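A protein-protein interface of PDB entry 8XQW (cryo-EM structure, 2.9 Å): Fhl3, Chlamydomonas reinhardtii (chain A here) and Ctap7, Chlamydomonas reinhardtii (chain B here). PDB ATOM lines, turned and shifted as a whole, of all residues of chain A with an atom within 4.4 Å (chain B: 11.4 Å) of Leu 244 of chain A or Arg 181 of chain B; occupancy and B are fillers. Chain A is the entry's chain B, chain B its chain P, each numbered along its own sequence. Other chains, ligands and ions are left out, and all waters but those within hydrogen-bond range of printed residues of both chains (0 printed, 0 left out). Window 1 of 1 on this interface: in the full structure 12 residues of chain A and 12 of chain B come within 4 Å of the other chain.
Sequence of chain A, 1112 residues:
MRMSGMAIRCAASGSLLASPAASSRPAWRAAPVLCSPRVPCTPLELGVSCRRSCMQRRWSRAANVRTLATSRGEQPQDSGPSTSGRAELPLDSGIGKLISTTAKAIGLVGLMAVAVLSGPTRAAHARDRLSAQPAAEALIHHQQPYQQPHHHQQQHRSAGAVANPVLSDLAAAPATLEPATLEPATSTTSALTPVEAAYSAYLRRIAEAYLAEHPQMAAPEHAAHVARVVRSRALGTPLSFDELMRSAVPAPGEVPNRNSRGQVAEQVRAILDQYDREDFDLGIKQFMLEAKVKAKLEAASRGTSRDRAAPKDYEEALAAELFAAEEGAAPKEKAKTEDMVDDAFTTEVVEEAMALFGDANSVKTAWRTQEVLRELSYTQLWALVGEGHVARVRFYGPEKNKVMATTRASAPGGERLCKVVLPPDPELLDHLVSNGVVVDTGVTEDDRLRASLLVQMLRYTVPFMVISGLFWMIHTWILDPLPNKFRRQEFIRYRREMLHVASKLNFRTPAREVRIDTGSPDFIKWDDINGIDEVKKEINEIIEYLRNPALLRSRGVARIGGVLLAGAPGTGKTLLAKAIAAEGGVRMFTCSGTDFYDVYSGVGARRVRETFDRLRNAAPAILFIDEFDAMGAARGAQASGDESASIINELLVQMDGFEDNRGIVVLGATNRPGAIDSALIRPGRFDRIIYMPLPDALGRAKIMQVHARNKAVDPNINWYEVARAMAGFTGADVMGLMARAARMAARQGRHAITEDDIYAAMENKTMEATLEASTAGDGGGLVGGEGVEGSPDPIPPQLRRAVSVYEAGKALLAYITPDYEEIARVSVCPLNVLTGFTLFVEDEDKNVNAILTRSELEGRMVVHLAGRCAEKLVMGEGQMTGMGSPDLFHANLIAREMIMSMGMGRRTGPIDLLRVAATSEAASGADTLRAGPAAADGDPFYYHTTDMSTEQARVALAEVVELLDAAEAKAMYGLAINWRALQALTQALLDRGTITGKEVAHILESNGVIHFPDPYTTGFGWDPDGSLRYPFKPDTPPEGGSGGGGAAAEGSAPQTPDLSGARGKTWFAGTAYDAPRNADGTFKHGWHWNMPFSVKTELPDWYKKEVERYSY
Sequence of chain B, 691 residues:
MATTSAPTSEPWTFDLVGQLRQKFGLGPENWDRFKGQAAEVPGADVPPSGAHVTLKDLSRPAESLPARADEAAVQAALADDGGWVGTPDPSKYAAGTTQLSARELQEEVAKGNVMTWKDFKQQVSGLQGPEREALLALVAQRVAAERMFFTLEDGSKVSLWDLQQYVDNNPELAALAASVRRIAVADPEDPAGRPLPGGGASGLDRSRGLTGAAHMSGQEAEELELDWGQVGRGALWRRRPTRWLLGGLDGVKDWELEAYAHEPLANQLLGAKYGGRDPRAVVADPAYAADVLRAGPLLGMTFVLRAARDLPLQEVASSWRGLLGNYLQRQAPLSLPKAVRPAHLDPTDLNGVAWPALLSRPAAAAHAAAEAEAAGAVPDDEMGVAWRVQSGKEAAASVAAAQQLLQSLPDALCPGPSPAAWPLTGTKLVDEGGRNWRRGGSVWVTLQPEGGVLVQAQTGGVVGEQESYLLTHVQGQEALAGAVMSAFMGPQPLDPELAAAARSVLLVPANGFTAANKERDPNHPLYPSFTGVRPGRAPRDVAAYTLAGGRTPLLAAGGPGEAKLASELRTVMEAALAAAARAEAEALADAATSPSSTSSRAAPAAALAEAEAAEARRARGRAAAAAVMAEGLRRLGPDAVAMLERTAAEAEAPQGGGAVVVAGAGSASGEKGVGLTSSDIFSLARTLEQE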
ATOM      1  N   SER A 240       4.735  10.182 -15.789  1.00  0.00           N
ATOM      2  CA  SER A 240       3.868  10.679 -14.740  1.00  0.00           C
ATOM      3  C   SER A 240       4.106  12.174 -14.563  1.00  0.00           C
ATOM      4  O   SER A 240       4.855  12.804 -15.312  1.00  0.00           O
ATOM      5  CB  SER A 240       4.119   9.923 -13.443  1.00  0.00           C
ATOM      6  OG  SER A 240       5.508   9.732 -13.243  1.00  0.00           O
ATOM      7  N   PHE A 241       3.467  12.757 -13.556  1.00  0.00           N
ATOM      8  CA  PHE A 241       3.691  14.173 -13.311  1.00  0.00           C
ATOM      9  C   PHE A 241       4.972  14.406 -12.531  1.00  0.00           C
ATOM     10  O   PHE A 241       5.689  15.374 -12.794  1.00  0.00           O
ATOM     11  CB  PHE A 241       2.511  14.782 -12.565  1.00  0.00           C
ATOM     12  CG  PHE A 241       2.653  16.249 -12.334  1.00  0.00           C
ATOM     13  CD1 PHE A 241       2.283  17.149 -13.311  1.00  0.00           C
ATOM     14  CD2 PHE A 241       3.168  16.729 -11.145  1.00  0.00           C
ATOM     15  CE1 PHE A 241       2.416  18.500 -13.105  1.00  0.00           C
ATOM     16  CE2 PHE A 241       3.303  18.079 -10.935  1.00  0.00           C
ATOM     17  CZ  PHE A 241       2.925  18.966 -11.916  1.00  0.00           C
ATOM     18  N   ASP A 242       5.272  13.537 -11.569  1.00  0.00           N
ATOM     19  CA  ASP A 242       6.455  13.721 -10.743  1.00  0.00           C
ATOM     20  C   ASP A 242       7.737  13.554 -11.539  1.00  0.00           C
ATOM     21  O   ASP A 242       8.776  14.089 -11.144  1.00  0.00           O
ATOM     22  CB  ASP A 242       6.428  12.740  -9.577  1.00  0.00           C
ATOM     23  CG  ASP A 242       5.260  12.983  -8.647  1.00  0.00           C
ATOM     24  OD1 ASP A 242       4.901  14.159  -8.442  1.00  0.00           O
ATOM     25  OD2 ASP A 242       4.698  11.998  -8.122  1.00  0.00           O
ATOM     26  N   GLU A 243       7.684  12.824 -12.648  1.00  0.00           N
ATOM     27  CA  GLU A 243       8.844  12.673 -13.514  1.00  0.00           C
ATOM     28  C   GLU A 243       8.907  13.728 -14.607  1.00  0.00           C
ATOM     29  O   GLU A 243       9.990  13.981 -15.139  1.00  0.00           O
ATOM     30  CB  GLU A 243       8.844  11.283 -14.145  1.00  0.00           C
ATOM     31  CG  GLU A 243       9.920  10.364 -13.608  1.00  0.00           C
ATOM     32  CD  GLU A 243      11.315  10.955 -13.716  1.00  0.00           C
ATOM     33  OE1 GLU A 243      11.626  11.574 -14.755  1.00  0.00           O
ATOM     34  OE2 GLU A 243      12.107  10.796 -12.765  1.00  0.00           O
ATOM     35  N   LEU A 244       7.782  14.348 -14.953  1.00  0.00           N
ATOM     36  CA  LEU A 244       7.805  15.398 -15.959  1.00  0.00           C
ATOM     37  C   LEU A 244       8.447  16.674 -15.434  1.00  0.00           C
ATOM     38  O   LEU A 244       9.123  17.378 -16.189  1.00  0.00           O
ATOM     39  CB  LEU A 244       6.389  15.690 -16.445  1.00  0.00           C
ATOM     40  CG  LEU A 244       6.214  16.943 -17.297  1.00  0.00           C
ATOM     41  CD1 LEU A 244       6.794  16.726 -18.675  1.00  0.00           C
ATOM     42  CD2 LEU A 244       4.758  17.320 -17.392  1.00  0.00           C
ATOM     43  N   MET A 245       8.267  16.979 -14.154  1.00  0.00           N
ATOM     44  CA  MET A 245       8.797  18.199 -13.570  1.00  0.00           C
ATOM     45  C   MET A 245      10.068  17.961 -12.770  1.00  0.00           C
ATOM     46  O   MET A 245      10.288  18.636 -11.760  1.00  0.00           O
ATOM     47  CB  MET A 245       7.741  18.861 -12.692  1.00  0.00           C
ATOM     48  CG  MET A 245       6.382  18.955 -13.347  1.00  0.00           C
ATOM     49  SD  MET A 245       5.657  20.601 -13.225  1.00  0.00           S
ATOM     50  CE  MET A 245       6.692  21.508 -14.368  1.00  0.00           C
ATOM     51  N   ARG A 246      10.905  17.021 -13.189  1.00  0.00           N
ATOM     52  CA  ARG A 246      12.197  16.800 -12.558  1.00  0.00           C
ATOM     53  C   ARG A 246      13.309  17.387 -13.419  1.00  0.00           C
ATOM     54  O   ARG A 246      13.205  17.466 -14.644  1.00  0.00           O
ATOM     55  CB  ARG A 246      12.438  15.314 -12.304  1.00  0.00           C
ATOM     56  CG  ARG A 246      13.147  14.588 -13.412  1.00  0.00           C
ATOM     57  CD  ARG A 246      13.865  13.385 -12.844  1.00  0.00           C
ATOM     58  NE  ARG A 246      14.329  13.648 -11.486  1.00  0.00           N
ATOM     59  CZ  ARG A 246      14.940  12.756 -10.715  1.00  0.00           C
ATOM     60  NH1 ARG A 246      15.168  11.530 -11.164  1.00  0.00           N
ATOM     61  NH2 ARG A 246      15.325  13.091  -9.493  1.00  0.00           N
ATOM     62  N   GLY A 386      15.787  26.465 -19.538  1.00  0.00           N
ATOM     63  CA  GLY A 386      14.656  25.897 -20.240  1.00  0.00           C
ATOM     64  C   GLY A 386      13.534  25.391 -19.367  1.00  0.00           C
ATOM     65  O   GLY A 386      12.472  25.052 -19.892  1.00  0.00           O
ATOM     66  N   GLU A 387      13.734  25.333 -18.054  1.00  0.00           N
ATOM     67  CA  GLU A 387      12.684  24.962 -17.118  1.00  0.00           C
ATOM     68  C   GLU A 387      12.249  26.136 -16.258  1.00  0.00           C
ATOM     69  O   GLU A 387      11.475  25.949 -15.317  1.00  0.00           O
ATOM     70  CB  GLU A 387      13.149  23.819 -16.219  1.00  0.00           C
ATOM     71  CG  GLU A 387      13.790  22.677 -16.961  1.00  0.00           C
ATOM     72  CD  GLU A 387      14.620  21.794 -16.053  1.00  0.00           C
ATOM     73  OE1 GLU A 387      15.406  20.977 -16.571  1.00  0.00           O
ATOM     74  OE2 GLU A 387      14.490  21.921 -14.820  1.00  0.00           O
ATOM     75  N   PRO B 171      -4.138  21.659  -8.620  1.00  0.00           N
ATOM     76  CA  PRO B 171      -2.892  22.328  -8.240  1.00  0.00           C
ATOM     77  C   PRO B 171      -1.743  21.994  -9.175  1.00  0.00           C
ATOM     78  O   PRO B 171      -0.786  22.767  -9.281  1.00  0.00           O
ATOM     79  CB  PRO B 171      -2.645  21.809  -6.819  1.00  0.00           C
ATOM     80  CG  PRO B 171      -3.257  20.446  -6.817  1.00  0.00           C
ATOM     81  CD  PRO B 171      -4.349  20.414  -7.864  1.00  0.00           C
ATOM     82  N   GLU B 172      -1.827  20.866  -9.882  1.00  0.00           N
ATOM     83  CA  GLU B 172      -0.738  20.502 -10.782  1.00  0.00           C
ATOM     84  C   GLU B 172      -0.716  21.405 -12.009  1.00  0.00           C
ATOM     85  O   GLU B 172       0.348  21.887 -12.411  1.00  0.00           O
ATOM     86  CB  GLU B 172      -0.833  19.025 -11.171  1.00  0.00           C
ATOM     87  CG  GLU B 172      -1.848  18.669 -12.248  1.00  0.00           C
ATOM     88  CD  GLU B 172      -3.136  18.122 -11.677  1.00  0.00           C
ATOM     89  OE1 GLU B 172      -3.359  18.280 -10.460  1.00  0.00           O
ATOM     90  OE2 GLU B 172      -3.925  17.531 -12.443  1.00  0.00           O
ATOM     91  N   LEU B 173      -1.878  21.677 -12.602  1.00  0.00           N
ATOM     92  CA  LEU B 173      -1.917  22.606 -13.721  1.00  0.00           C
ATOM     93  C   LEU B 173      -1.626  24.025 -13.261  1.00  0.00           C
ATOM     94  O   LEU B 173      -1.037  24.813 -14.008  1.00  0.00           O
ATOM     95  CB  LEU B 173      -3.267  22.529 -14.417  1.00  0.00           C
ATOM     96  CG  LEU B 173      -3.300  21.578 -15.607  1.00  0.00           C
ATOM     97  CD1 LEU B 173      -4.722  21.147 -15.893  1.00  0.00           C
ATOM     98  CD2 LEU B 173      -2.680  22.244 -16.821  1.00  0.00           C
ATOM     99  N   ALA B 174      -2.010  24.358 -12.029  1.00  0.00           N
ATOM    100  CA  ALA B 174      -1.634  25.649 -11.472  1.00  0.00           C
ATOM    101  C   ALA B 174      -0.122  25.783 -11.391  1.00  0.00           C
ATOM    102  O   ALA B 174       0.437  26.823 -11.752  1.00  0.00           O
ATOM    103  CB  ALA B 174      -2.269  25.833 -10.096  1.00  0.00           C
ATOM    104  N   ALA B 175       0.561  24.733 -10.932  1.00  0.00           N
ATOM    105  CA  ALA B 175       2.014  24.796 -10.829  1.00  0.00           C
ATOM    106  C   ALA B 175       2.668  24.789 -12.202  1.00  0.00           C
ATOM    107  O   ALA B 175       3.728  25.393 -12.393  1.00  0.00           O
ATOM    108  CB  ALA B 175       2.532  23.636  -9.982  1.00  0.00           C
ATOM    109  N   LEU B 176       2.060  24.100 -13.166  1.00  0.00           N
ATOM    110  CA  LEU B 176       2.595  24.113 -14.521  1.00  0.00           C
ATOM    111  C   LEU B 176       2.511  25.507 -15.120  1.00  0.00           C
ATOM    112  O   LEU B 176       3.458  25.985 -15.754  1.00  0.00           O
ATOM    113  CB  LEU B 176       1.849  23.106 -15.390  1.00  0.00           C
ATOM    114  CG  LEU B 176       2.719  21.982 -15.939  1.00  0.00           C
ATOM    115  CD1 LEU B 176       1.889  21.028 -16.763  1.00  0.00           C
ATOM    116  CD2 LEU B 176       3.842  22.568 -16.765  1.00  0.00           C
ATOM    117  N   ALA B 177       1.379  26.182 -14.922  1.00  0.00           N
ATOM    118  CA  ALA B 177       1.257  27.568 -15.350  1.00  0.00           C
ATOM    119  C   ALA B 177       2.147  28.502 -14.542  1.00  0.00           C
ATOM    120  O   ALA B 177       2.498  29.577 -15.033  1.00  0.00           O
ATOM    121  CB  ALA B 177      -0.196  28.021 -15.245  1.00  0.00           C
ATOM    122  N   ALA B 178       2.500  28.121 -13.313  1.00  0.00           N
ATOM    123  CA  ALA B 178       3.380  28.954 -12.500  1.00  0.00           C
ATOM    124  C   ALA B 178       4.728  29.138 -13.176  1.00  0.00           C
ATOM    125  O   ALA B 178       5.258  30.253 -13.242  1.00  0.00           O
ATOM    126  CB  ALA B 178       3.549  28.337 -11.113  1.00  0.00           C
ATOM    127  N   SER B 179       5.305  28.052 -13.678  1.00  0.00           N
ATOM    128  CA  SER B 179       6.464  28.134 -14.553  1.00  0.00           C
ATOM    129  C   SER B 179       5.971  28.460 -15.961  1.00  0.00           C
ATOM    130  O   SER B 179       4.779  28.670 -16.197  1.00  0.00           O
ATOM    131  CB  SER B 179       7.262  26.837 -14.502  1.00  0.00           C
ATOM    132  OG  SER B 179       6.924  25.991 -15.585  1.00  0.00           O
ATOM    133  N   VAL B 180       6.880  28.506 -16.923  1.00  0.00           N
ATOM    134  CA  VAL B 180       6.501  28.788 -18.299  1.00  0.00           C
ATOM    135  C   VAL B 180       6.934  27.689 -19.257  1.00  0.00           C
ATOM    136  O   VAL B 180       6.743  27.844 -20.474  1.00  0.00           O
ATOM    137  CB  VAL B 180       7.054  30.155 -18.756  1.00  0.00           C
ATOM    138  CG1 VAL B 180       8.543  30.056 -19.079  1.00  0.00           C
ATOM    139  CG2 VAL B 180       6.240  30.717 -19.920  1.00  0.00           C
ATOM    140  N   ARG B 181       7.503  26.594 -18.754  1.00  0.00           N
ATOM    141  CA  ARG B 181       8.106  25.562 -19.590  1.00  0.00           C
ATOM    142  C   ARG B 181       7.260  25.262 -20.814  1.00  0.00           C
ATOM    143  O   ARG B 181       6.076  24.936 -20.703  1.00  0.00           O
ATOM    144  CB  ARG B 181       8.308  24.292 -18.769  1.00  0.00           C
ATOM    145  CG  ARG B 181       8.809  23.137 -19.597  1.00  0.00           C
ATOM    146  CD  ARG B 181       8.763  21.845 -18.830  1.00  0.00           C
ATOM    147  NE  ARG B 181       9.262  22.010 -17.476  1.00  0.00           N
ATOM    148  CZ  ARG B 181      10.025  21.119 -16.861  1.00  0.00           C
ATOM    149  NH1 ARG B 181      10.376  20.008 -17.491  1.00  0.00           N
ATOM    150  NH2 ARG B 181      10.445  21.339 -15.623  1.00  0.00           N
ATOM    151  N   ARG B 182       7.871  25.391 -21.984  1.00  0.00           N
ATOM    152  CA  ARG B 182       7.171  25.229 -23.249  1.00  0.00           C
ATOM    153  C   ARG B 182       7.354  23.801 -23.742  1.00  0.00           C
ATOM    154  O   ARG B 182       8.439  23.430 -24.198  1.00  0.00           O
ATOM    155  CB  ARG B 182       7.686  26.232 -24.277  1.00  0.00           C
ATOM    156  CG  ARG B 182       6.613  26.726 -25.226  1.00  0.00           C
ATOM    157  CD  ARG B 182       6.931  28.107 -25.770  1.00  0.00           C
ATOM    158  NE  ARG B 182       8.350  28.270 -26.065  1.00  0.00           N
ATOM    159  CZ  ARG B 182       9.151  29.115 -25.426  1.00  0.00           C
ATOM    160  NH1 ARG B 182       8.674  29.876 -24.451  1.00  0.00           N
ATOM    161  NH2 ARG B 182      10.430  29.196 -25.759  1.00  0.00           N
ATOM    162  N   ILE B 183       6.291  23.010 -23.658  1.00  0.00           N
ATOM    163  CA  ILE B 183       6.312  21.600 -24.021  1.00  0.00           C
ATOM    164  C   ILE B 183       5.701  21.458 -25.402  1.00  0.00           C
ATOM    165  O   ILE B 183       4.508  21.717 -25.589  1.00  0.00           O
ATOM    166  CB  ILE B 183       5.550  20.750 -22.995  1.00  0.00           C
ATOM    167  CG1 ILE B 183       6.185  20.900 -21.619  1.00  0.00           C
ATOM    168  CG2 ILE B 183       5.539  19.303 -23.407  1.00  0.00           C
ATOM    169  CD1 ILE B 183       5.366  20.296 -20.524  1.00  0.00           C
ATOM    170  N   ALA B 184       6.515  21.051 -26.372  1.00  0.00           N
ATOM    171  CA  ALA B 184       6.021  20.836 -27.719  1.00  0.00           C
ATOM    172  C   ALA B 184       4.937  19.768 -27.719  1.00  0.00           C
ATOM    173  O   ALA B 184       4.815  18.969 -26.791  1.00  0.00           O
ATOM    174  CB  ALA B 184       7.157  20.427 -28.651  1.00  0.00           C
ATOM    175  N   VAL B 185       4.136  19.764 -28.779  1.00  0.00           N
ATOM    176  CA  VAL B 185       3.014  18.846 -28.913  1.00  0.00           C
ATOM    177  C   VAL B 185       3.257  17.964 -30.127  1.00  0.00           C
ATOM    178  O   VAL B 185       3.812  18.419 -31.133  1.00  0.00           O
ATOM    179  CB  VAL B 185       1.676  19.601 -29.014  1.00  0.00           C
ATOM    180  CG1 VAL B 185       1.572  20.343 -30.320  1.00  0.00           C
ATOM    181  CG2 VAL B 185       0.515  18.649 -28.853  1.00  0.00           C
ATOM    182  N   GLY B 199       5.699  26.068 -32.864  1.00  0.00           N
ATOM    183  CA  GLY B 199       6.747  26.875 -32.263  1.00  0.00           C
ATOM    184  C   GLY B 199       6.171  28.111 -31.600  1.00  0.00           C
ATOM    185  O   GLY B 199       5.310  28.029 -30.718  1.00  0.00           O
ATOM    186  N   GLY B 200       6.653  29.275 -32.026  1.00  0.00           N
ATOM    187  CA  GLY B 200       6.113  30.534 -31.552  1.00  0.00           C
ATOM    188  C   GLY B 200       6.753  31.040 -30.278  1.00  0.00           C
ATOM    189  O   GLY B 200       7.083  30.255 -29.382  1.00  0.00           O
ATOM    190  N   ALA B 201       6.928  32.358 -30.183  1.00  0.00           N
ATOM    191  CA  ALA B 201       7.517  32.978 -29.006  1.00  0.00           C
ATOM    192  C   ALA B 201       6.518  33.732 -28.145  1.00  0.00           C
ATOM    193  O   ALA B 201       6.800  33.950 -26.963  1.00  0.00           O
ATOM    194  CB  ALA B 201       8.637  33.942 -29.414  1.00  0.00           C
ATOM    195  N   SER B 202       5.370  34.135 -28.698  1.00  0.00           N
ATOM    196  CA  SER B 202       4.287  34.742 -27.927  1.00  0.00           C
ATOM    197  C   SER B 202       4.762  36.015 -27.221  1.00  0.00           C
ATOM    198  O   SER B 202       4.931  36.063 -26.003  1.00  0.00           O
ATOM    199  CB  SER B 202       3.699  33.743 -26.925  1.00  0.00           C
ATOM    200  OG  SER B 202       3.248  34.410 -25.761  1.00  0.00           O
ATOM    201  N   ASP B 205       4.941  36.676 -23.613  1.00  0.00           N
ATOM    202  CA  ASP B 205       5.859  35.906 -22.781  1.00  0.00           C
ATOM    203  C   ASP B 205       7.314  36.237 -23.058  1.00  0.00           C
ATOM    204  O   ASP B 205       8.142  36.141 -22.149  1.00  0.00           O
ATOM    205  CB  ASP B 205       5.635  34.409 -22.983  1.00  0.00           C
ATOM    206  CG  ASP B 205       4.171  34.034 -22.967  1.00  0.00           C
ATOM    207  OD1 ASP B 205       3.349  34.870 -22.537  1.00  0.00           O
ATOM    208  OD2 ASP B 205       3.840  32.905 -23.380  1.00  0.00           O
ATOM    209  N   ARG B 208       8.573  39.144 -20.344  1.00  0.00           N
ATOM    210  CA  ARG B 208       8.963  39.081 -18.944  1.00  0.00           C
ATOM    211  C   ARG B 208      10.445  39.394 -18.821  1.00  0.00           C
ATOM    212  O   ARG B 208      11.207  39.263 -19.779  1.00  0.00           O
ATOM    213  CB  ARG B 208       8.659  37.710 -18.362  1.00  0.00           C
ATOM    214  CG  ARG B 208       7.188  37.430 -18.230  1.00  0.00           C
ATOM    215  CD  ARG B 208       6.847  36.047 -18.723  1.00  0.00           C
ATOM    216  NE  ARG B 208       7.329  35.021 -17.810  1.00  0.00           N
ATOM    217  CZ  ARG B 208       7.837  33.861 -18.206  1.00  0.00           C
ATOM    218  NH1 ARG B 208       7.928  33.583 -19.496  1.00  0.00           N
ATOM    219  NH2 ARG B 208       8.255  32.980 -17.309  1.00  0.00           N
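NH1 of Arg 181 of chain B is in hydrogen-bond range of O of Leu 244 of chain A (3.2 Å).
The backbone NH of Arg 181 of chain B lies within hydrogen-bond range of the side-chain hydroxyl of Ser 179 of chain B, at 3.3 Å. The backbone carbonyl oxygen of Leu 176 of chain B is in hydrogen-bond range of the side-chain hydroxyl of Ser 179 of chain B (3.5 Å).
Among the printed residues, merely in contact across the chains: Phe 241 of chain A with Glu 172 of chain B (3.8 Å), Met 245 of chain A with Leu 176 of chain B (3.9 Å), Met 245 of chain A with Arg 181 of chain B (3.96 Å) and Glu 387 of chain A with Arg 181 of chain B (3.7 Å).
Leu 244 of chain A touches one residue of chain B. Of chain A, only Leu 244 (3.2 Å), Met 245 (3.96 Å) and Glu 387 (3.7 Å) come within 4 Å of Arg 181 of chain B. No residue of chain B comes within 4 Å of Ser 240 of chain A. Phe 241 of chain A touches just one residue of chain B: Glu 172. Glu 243 of chain A touches none of the printed residues of chain B. Printed residues of chain A within 4 Å of Glu 172 of chain B: Phe 241. Of the printed residues of chain A, Leu 176 of chain B touches Met 245 (3.9 Å). The nearest residue of chain B that does not touch Leu 244 of chain A is Ile 183 of chain B (4.3 Å). The nearest printed residue of chain A that does not touch Leu 176 of chain B is Phe 241 of chain A (4.5 Å).
Along chain B the printed residues that touch a printed residue of chain A span positions 172 to 181. Of the 9 printed residues of chain A, 4 touch a printed residue of chain B. Printed residues of chain A that touch a printed residue of chain B: Phe 241, Leu 244, Met 245 and Glu 387. Among the printed residues, 5 pairs touch across the chains. Among the printed residues, no Asp or Glu carboxylate lies within 4 Å of a Lys or Arg side-chain nitrogen of the other chain.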
